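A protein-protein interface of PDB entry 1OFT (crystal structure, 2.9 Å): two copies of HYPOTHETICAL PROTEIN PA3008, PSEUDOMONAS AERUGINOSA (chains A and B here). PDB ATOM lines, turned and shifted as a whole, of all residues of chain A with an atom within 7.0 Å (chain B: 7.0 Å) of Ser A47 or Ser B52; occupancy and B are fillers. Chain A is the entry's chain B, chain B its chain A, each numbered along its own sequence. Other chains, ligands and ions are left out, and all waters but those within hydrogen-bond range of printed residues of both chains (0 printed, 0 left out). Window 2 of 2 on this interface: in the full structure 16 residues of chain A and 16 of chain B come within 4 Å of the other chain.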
ATOM      1  N   PRO A  43      -3.039   1.069  16.363  1.00  0.00           N
ATOM      2  CA  PRO A  43      -3.993   1.617  15.363  1.00  0.00           C
ATOM      3  C   PRO A  43      -3.674   3.055  14.939  1.00  0.00           C
ATOM      4  O   PRO A  43      -2.560   3.555  15.168  1.00  0.00           O
ATOM      5  CB  PRO A  43      -5.393   1.527  15.962  1.00  0.00           C
ATOM      6  CG  PRO A  43      -5.097   1.449  17.433  1.00  0.00           C
ATOM      7  CD  PRO A  43      -3.778   0.659  17.567  1.00  0.00           C
ATOM      8  N   ALA A  44      -4.642   3.713  14.302  1.00  0.00           N
ATOM      9  CA  ALA A  44      -4.449   5.084  13.833  1.00  0.00           C
ATOM     10  C   ALA A  44      -5.003   6.086  14.831  1.00  0.00           C
ATOM     11  O   ALA A  44      -5.902   5.765  15.599  1.00  0.00           O
ATOM     12  CB  ALA A  44      -5.115   5.270  12.485  1.00  0.00           C
ATOM     13  N   ALA A  45      -4.452   7.297  14.824  1.00  0.00           N
ATOM     14  CA  ALA A  45      -4.890   8.352  15.730  1.00  0.00           C
ATOM     15  C   ALA A  45      -4.781   7.939  17.202  1.00  0.00           C
ATOM     16  O   ALA A  45      -5.331   8.590  18.084  1.00  0.00           O
ATOM     17  CB  ALA A  45      -6.315   8.745  15.396  1.00  0.00           C
ATOM     18  N   PHE A  46      -4.072   6.849  17.465  1.00  0.00           N
ATOM     19  CA  PHE A  46      -3.886   6.383  18.832  1.00  0.00           C
ATOM     20  C   PHE A  46      -2.406   6.139  19.154  1.00  0.00           C
ATOM     21  O   PHE A  46      -1.618   5.751  18.274  1.00  0.00           O
ATOM     22  CB  PHE A  46      -4.667   5.097  19.065  1.00  0.00           C
ATOM     23  CG  PHE A  46      -4.595   4.613  20.478  1.00  0.00           C
ATOM     24  CD1 PHE A  46      -5.422   5.165  21.455  1.00  0.00           C
ATOM     25  CD2 PHE A  46      -3.676   3.645  20.849  1.00  0.00           C
ATOM     26  CE1 PHE A  46      -5.328   4.753  22.793  1.00  0.00           C
ATOM     27  CE2 PHE A  46      -3.576   3.226  22.180  1.00  0.00           C
ATOM     28  CZ  PHE A  46      -4.402   3.781  23.156  1.00  0.00           C
ATOM     29  N   SER A  47      -2.031   6.401  20.404  1.00  0.00           N
ATOM     30  CA  SER A  47      -0.662   6.199  20.883  1.00  0.00           C
ATOM     31  C   SER A  47      -0.707   6.090  22.379  1.00  0.00           C
ATOM     32  O   SER A  47      -1.574   6.668  23.024  1.00  0.00           O
ATOM     33  CB  SER A  47       0.302   7.338  20.495  1.00  0.00           C
ATOM     34  OG  SER A  47      -0.333   8.476  19.950  1.00  0.00           O
ATOM     35  N   GLU A  48       0.227   5.339  22.937  1.00  0.00           N
ATOM     36  CA  GLU A  48       0.244   5.146  24.368  1.00  0.00           C
ATOM     37  C   GLU A  48       1.606   5.492  24.915  1.00  0.00           C
ATOM     38  O   GLU A  48       2.628   5.132  24.328  1.00  0.00           O
ATOM     39  CB  GLU A  48      -0.111   3.701  24.697  1.00  0.00           C
ATOM     40  CG  GLU A  48      -0.540   3.485  26.143  1.00  0.00           C
ATOM     41  CD  GLU A  48      -1.243   2.142  26.355  1.00  0.00           C
ATOM     42  OE1 GLU A  48      -1.912   1.968  27.398  1.00  0.00           O
ATOM     43  OE2 GLU A  48      -1.127   1.257  25.481  1.00  0.00           O
ATOM     44  N   LEU A  49       1.602   6.206  26.038  1.00  0.00           N
ATOM     45  CA  LEU A  49       2.817   6.654  26.703  1.00  0.00           C
ATOM     46  C   LEU A  49       2.813   6.013  28.076  1.00  0.00           C
ATOM     47  O   LEU A  49       1.844   6.178  28.828  1.00  0.00           O
ATOM     48  CB  LEU A  49       2.783   8.171  26.853  1.00  0.00           C
ATOM     49  CG  LEU A  49       4.034   8.972  27.225  1.00  0.00           C
ATOM     50  CD1 LEU A  49       3.589  10.359  27.670  1.00  0.00           C
ATOM     51  CD2 LEU A  49       4.812   8.311  28.352  1.00  0.00           C
ATOM     52  N   SER A  50       3.882   5.285  28.395  1.00  0.00           N
ATOM     53  CA  SER A  50       4.006   4.607  29.686  1.00  0.00           C
ATOM     54  C   SER A  50       5.162   5.203  30.456  1.00  0.00           C
ATOM     55  O   SER A  50       6.247   5.390  29.905  1.00  0.00           O
ATOM     56  CB  SER A  50       4.268   3.114  29.498  1.00  0.00           C
ATOM     57  OG  SER A  50       3.311   2.529  28.639  1.00  0.00           O
ATOM     58  N   ARG A 141      -8.988   0.258  22.461  1.00  0.00           N
ATOM     59  CA  ARG A 141      -8.142   1.062  21.594  1.00  0.00           C
ATOM     60  C   ARG A 141      -8.846   1.340  20.282  1.00  0.00           C
ATOM     61  O   ARG A 141      -9.015   2.493  19.903  1.00  0.00           O
ATOM     62  CB  ARG A 141      -6.809   0.369  21.339  1.00  0.00           C
ATOM     63  CG  ARG A 141      -6.047   0.096  22.613  1.00  0.00           C
ATOM     64  CD  ARG A 141      -4.676  -0.506  22.371  1.00  0.00           C
ATOM     65  NE  ARG A 141      -4.062  -0.849  23.648  1.00  0.00           N
ATOM     66  CZ  ARG A 141      -2.757  -0.812  23.890  1.00  0.00           C
ATOM     67  NH1 ARG A 141      -2.305  -1.137  25.094  1.00  0.00           N
ATOM     68  NH2 ARG A 141      -1.906  -0.448  22.933  1.00  0.00           N
ATOM     69  N   GLN A 154      -6.591  13.309  18.098  1.00  0.00           N
ATOM     70  CA  GLN A 154      -5.577  12.355  18.512  1.00  0.00           C
ATOM     71  C   GLN A 154      -5.902  11.748  19.870  1.00  0.00           C
ATOM     72  O   GLN A 154      -6.250  12.453  20.809  1.00  0.00           O
ATOM     73  CB  GLN A 154      -4.219  13.051  18.629  1.00  0.00           C
ATOM     74  CG  GLN A 154      -3.464  13.216  17.354  1.00  0.00           C
ATOM     75  CD  GLN A 154      -3.367  11.917  16.603  1.00  0.00           C
ATOM     76  OE1 GLN A 154      -4.292  11.541  15.885  1.00  0.00           O
ATOM     77  NE2 GLN A 154      -2.258  11.200  16.781  1.00  0.00           N
ATOM     78  N   SER A 155      -5.764  10.435  19.991  1.00  0.00           N
ATOM     79  CA  SER A 155      -6.009   9.791  21.268  1.00  0.00           C
ATOM     80  C   SER A 155      -4.671   9.399  21.852  1.00  0.00           C
ATOM     81  O   SER A 155      -3.883   8.732  21.183  1.00  0.00           O
ATOM     82  CB  SER A 155      -6.850   8.540  21.108  1.00  0.00           C
ATOM     83  OG  SER A 155      -7.027   7.935  22.374  1.00  0.00           O
ATOM     84  N   LEU A 156      -4.413   9.826  23.086  1.00  0.00           N
ATOM     85  CA  LEU A 156      -3.158   9.529  23.765  1.00  0.00           C
ATOM     86  C   LEU A 156      -3.510   8.930  25.088  1.00  0.00           C
ATOM     87  O   LEU A 156      -4.214   9.553  25.875  1.00  0.00           O
ATOM     88  CB  LEU A 156      -2.352  10.799  24.007  1.00  0.00           C
ATOM     89  CG  LEU A 156      -1.061  10.648  24.819  1.00  0.00           C
ATOM     90  CD1 LEU A 156      -0.054   9.877  24.003  1.00  0.00           C
ATOM     91  CD2 LEU A 156      -0.482  12.012  25.176  1.00  0.00           C
ATOM     92  N   ASN A 157      -3.039   7.715  25.338  1.00  0.00           N
ATOM     93  CA  ASN A 157      -3.325   7.060  26.604  1.00  0.00           C
ATOM     94  C   ASN A 157      -2.049   6.969  27.435  1.00  0.00           C
ATOM     95  O   ASN A 157      -1.011   6.494  26.970  1.00  0.00           O
ATOM     96  CB  ASN A 157      -3.913   5.677  26.365  1.00  0.00           C
ATOM     97  CG  ASN A 157      -4.482   5.074  27.621  1.00  0.00           C
ATOM     98  OD1 ASN A 157      -5.246   5.718  28.346  1.00  0.00           O
ATOM     99  ND2 ASN A 157      -4.115   3.832  27.891  1.00  0.00           N
ATOM    100  N   ILE A 158      -2.139   7.444  28.671  1.00  0.00           N
ATOM    101  CA  ILE A 158      -1.006   7.472  29.577  1.00  0.00           C
ATOM    102  C   ILE A 158      -1.107   6.494  30.730  1.00  0.00           C
ATOM    103  O   ILE A 158      -2.020   6.579  31.560  1.00  0.00           O
ATOM    104  CB  ILE A 158      -0.842   8.866  30.154  1.00  0.00           C
ATOM    105  CG1 ILE A 158      -0.434   9.816  29.029  1.00  0.00           C
ATOM    106  CG2 ILE A 158       0.159   8.837  31.293  1.00  0.00           C
ATOM    107  CD1 ILE A 158      -0.350  11.277  29.417  1.00  0.00           C
ATOM    108  N   SER B  50       8.002   4.773  27.707  1.00  0.00           N
ATOM    109  CA  SER B  50       7.700   3.915  26.567  1.00  0.00           C
ATOM    110  C   SER B  50       6.750   4.626  25.627  1.00  0.00           C
ATOM    111  O   SER B  50       5.749   5.203  26.060  1.00  0.00           O
ATOM    112  CB  SER B  50       7.053   2.611  27.036  1.00  0.00           C
ATOM    113  OG  SER B  50       7.842   1.970  28.028  1.00  0.00           O
ATOM    114  N   LEU B  51       7.052   4.577  24.338  1.00  0.00           N
ATOM    115  CA  LEU B  51       6.209   5.226  23.348  1.00  0.00           C
ATOM    116  C   LEU B  51       5.821   4.270  22.238  1.00  0.00           C
ATOM    117  O   LEU B  51       6.679   3.693  21.574  1.00  0.00           O
ATOM    118  CB  LEU B  51       6.940   6.426  22.757  1.00  0.00           C
ATOM    119  CG  LEU B  51       7.092   7.580  23.735  1.00  0.00           C
ATOM    120  CD1 LEU B  51       8.183   8.523  23.251  1.00  0.00           C
ATOM    121  CD2 LEU B  51       5.739   8.285  23.877  1.00  0.00           C
ATOM    122  N   SER B  52       4.520   4.106  22.038  1.00  0.00           N
ATOM    123  CA  SER B  52       4.031   3.235  20.982  1.00  0.00           C
ATOM    124  C   SER B  52       3.041   3.990  20.103  1.00  0.00           C
ATOM    125  O   SER B  52       2.222   4.754  20.591  1.00  0.00           O
ATOM    126  CB  SER B  52       3.369   1.990  21.578  1.00  0.00           C
ATOM    127  OG  SER B  52       2.282   2.337  22.421  1.00  0.00           O
ATOM    128  N   GLY B  53       3.128   3.763  18.802  1.00  0.00           N
ATOM    129  CA  GLY B  53       2.254   4.421  17.860  1.00  0.00           C
ATOM    130  C   GLY B  53       3.122   4.728  16.668  1.00  0.00           C
ATOM    131  O   GLY B  53       4.272   4.298  16.641  1.00  0.00           O
ATOM    132  N   LEU B  54       2.593   5.446  15.681  1.00  0.00           N
ATOM    133  CA  LEU B  54       3.383   5.810  14.506  1.00  0.00           C
ATOM    134  C   LEU B  54       4.805   6.201  14.922  1.00  0.00           C
ATOM    135  O   LEU B  54       5.001   7.027  15.814  1.00  0.00           O
ATOM    136  CB  LEU B  54       2.735   6.991  13.783  1.00  0.00           C
ATOM    137  CG  LEU B  54       1.798   6.640  12.645  1.00  0.00           C
ATOM    138  CD1 LEU B  54       2.621   5.945  11.569  1.00  0.00           C
ATOM    139  CD2 LEU B  54       0.672   5.745  13.147  1.00  0.00           C
ATOM    140  N   PRO B  55       5.821   5.611  14.283  1.00  0.00           N
ATOM    141  CA  PRO B  55       7.197   5.964  14.652  1.00  0.00           C
ATOM    142  C   PRO B  55       7.404   7.482  14.628  1.00  0.00           C
ATOM    143  O   PRO B  55       8.138   8.032  15.448  1.00  0.00           O
ATOM    144  CB  PRO B  55       8.024   5.259  13.587  1.00  0.00           C
ATOM    145  CG  PRO B  55       7.100   5.298  12.386  1.00  0.00           C
ATOM    146  CD  PRO B  55       5.789   4.876  13.008  1.00  0.00           C
ATOM    147  N   HIS B  57       4.963  10.001  14.978  1.00  0.00           N
ATOM    148  CA  HIS B  57       4.279  10.652  16.077  1.00  0.00           C
ATOM    149  C   HIS B  57       4.904  10.385  17.446  1.00  0.00           C
ATOM    150  O   HIS B  57       4.651  11.131  18.380  1.00  0.00           O
ATOM    151  CB  HIS B  57       2.798  10.279  16.097  1.00  0.00           C
ATOM    152  CG  HIS B  57       1.983  11.163  16.982  1.00  0.00           C
ATOM    153  ND1 HIS B  57       1.558  10.777  18.235  1.00  0.00           N
ATOM    154  CD2 HIS B  57       1.583  12.448  16.826  1.00  0.00           C
ATOM    155  CE1 HIS B  57       0.934  11.787  18.815  1.00  0.00           C
ATOM    156  NE2 HIS B  57       0.936  12.813  17.982  1.00  0.00           N
ATOM    157  N   CYS B  58       5.703   9.330  17.580  1.00  0.00           N
ATOM    158  CA  CYS B  58       6.361   9.040  18.851  1.00  0.00           C
ATOM    159  C   CYS B  58       7.519  10.009  19.041  1.00  0.00           C
ATOM    160  O   CYS B  58       7.773  10.458  20.159  1.00  0.00           O
ATOM    161  CB  CYS B  58       6.863   7.599  18.879  1.00  0.00           C
ATOM    162  SG  CYS B  58       5.488   6.407  18.967  1.00  0.00           S
ATOM    163  N   LEU B  61       6.159  13.259  20.300  1.00  0.00           N
ATOM    164  CA  LEU B  61       5.863  13.224  21.719  1.00  0.00           C
ATOM    165  C   LEU B  61       7.128  13.255  22.530  1.00  0.00           C
ATOM    166  O   LEU B  61       7.100  13.618  23.702  1.00  0.00           O
ATOM    167  CB  LEU B  61       5.099  11.953  22.067  1.00  0.00           C
ATOM    168  CG  LEU B  61       3.605  12.084  22.343  1.00  0.00           C
ATOM    169  CD1 LEU B  61       2.999  13.180  21.500  1.00  0.00           C
ATOM    170  CD2 LEU B  61       2.932  10.746  22.060  1.00  0.00           C
ATOM    171  N   ARG B 159      12.004   3.519  25.440  1.00  0.00           N
ATOM    172  CA  ARG B 159      11.687   2.368  24.602  1.00  0.00           C
ATOM    173  C   ARG B 159      10.777   2.792  23.477  1.00  0.00           C
ATOM    174  O   ARG B 159       9.564   2.806  23.638  1.00  0.00           O
ATOM    175  CB  ARG B 159      10.974   1.293  25.413  1.00  0.00           C
ATOM    176  CG  ARG B 159      11.799   0.749  26.545  1.00  0.00           C
ATOM    177  CD  ARG B 159      10.936  -0.031  27.479  1.00  0.00           C
ATOM    178  NE  ARG B 159      10.318  -1.162  26.808  1.00  0.00           N
ATOM    179  CZ  ARG B 159       9.437  -1.964  27.391  1.00  0.00           C
ATOM    180  NH1 ARG B 159       8.917  -2.980  26.714  1.00  0.00           N
ATOM    181  NH2 ARG B 159       9.077  -1.747  28.654  1.00  0.00           N
ATOM    182  N   LEU B 160      11.365   3.158  22.347  1.00  0.00           N
ATOM    183  CA  LEU B 160      10.582   3.560  21.196  1.00  0.00           C
ATOM    184  C   LEU B 160      10.039   2.297  20.538  1.00  0.00           C
ATOM    185  O   LEU B 160      10.633   1.218  20.657  1.00  0.00           O
ATOM    186  CB  LEU B 160      11.437   4.353  20.204  1.00  0.00           C
ATOM    187  CG  LEU B 160      11.614   5.851  20.479  1.00  0.00           C
ATOM    188  CD1 LEU B 160      12.485   6.476  19.405  1.00  0.00           C
ATOM    189  CD2 LEU B 160      10.251   6.535  20.498  1.00  0.00           C
ATOM    190  N   GLY B 161       8.907   2.435  19.854  1.00  0.00           N
ATOM    191  CA  GLY B 161       8.298   1.289  19.207  1.00  0.00           C
ATOM    192  C   GLY B 161       7.697   0.359  20.245  1.00  0.00           C
ATOM    193  O   GLY B 161       6.490   0.052  20.132  1.00  0.00           O
ATOM    194  OXT GLY B 161       8.429  -0.062  21.172  1.00  0.00           O
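ND1 of His B57 sits at hydrogen-bond distance from OG of Ser A47, at 3.4 Å.
The backbone NH (N) of Glu A48 lies within hydrogen-bond range of the backbone carbonyl oxygen (O) of Ser B52, at 3.1 Å.
N of Ser B50 lies within hydrogen-bond range of O of Ser A50, 2.9 Å away.
OE2 of Glu A48 is in salt-bridge range of NH1 of Arg A141, at 2.7 Å.
O of Leu B51 lies within hydrogen-bond range of N of Gly B161 (3.1 Å).
The backbone carbonyl oxygen of Ser A155 is in hydrogen-bond range of the backbone NH of Ser A47 (3.1 Å).
N of Leu A49 sits at hydrogen-bond distance from O of Asn A157, at 2.8 Å.
The backbone NH (N) of Asn A157 lies within hydrogen-bond range of the backbone carbonyl oxygen (O) of Ser A47 (2.9 Å).
The backbone carbonyl oxygen (O) of Arg B159 is in hydrogen-bond range of the backbone NH (N) of Leu B51 (3.2 Å).
Ser A47 touches Ser B52.
Ser B50 touches Glu A48 (O to O, 3.6 Å).
Leu B51 touches Glu A48.
CA of Leu A49 touches O of Ser B50, at 3.3 Å.
Leu A49 touches Leu B51 (CG to CD2, 3.8 Å).
His B57 touches Gln A154 (NE2 to NE2, 3.8 Å).
CD1 of Leu A156 touches CD2 of Leu B61, at 3.7 Å.
Of chain B, only Ser B52 (3.2 Å) and His B57 (3.4 Å) come within 4 Å of Ser A47.
Of the printed residues of chain B, Glu A48 touches Ser B50, Leu B51 and Ser B52.
Ile A158 touches none of the printed residues of chain B.
Of the printed residues of chain A, Ser B50 touches Glu A48, Leu A49 and Ser A50.
Ser B52 touches two residues of chain A.
The nearest residue of chain B that does not touch Ser A47 is Gly B53 (4.4 Å).
Of the 14 printed residues of chain A, 6 touch a printed residue of chain B.
Among the printed residues, 10 pairs touch across the chains.
Ser A50 touches its own counterpart, Ser B50.
1 position is printed for both chains.
Of the 10 pairs that touch across the chains among the printed residues, 1 has its exchanged pair printed and touching as well.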
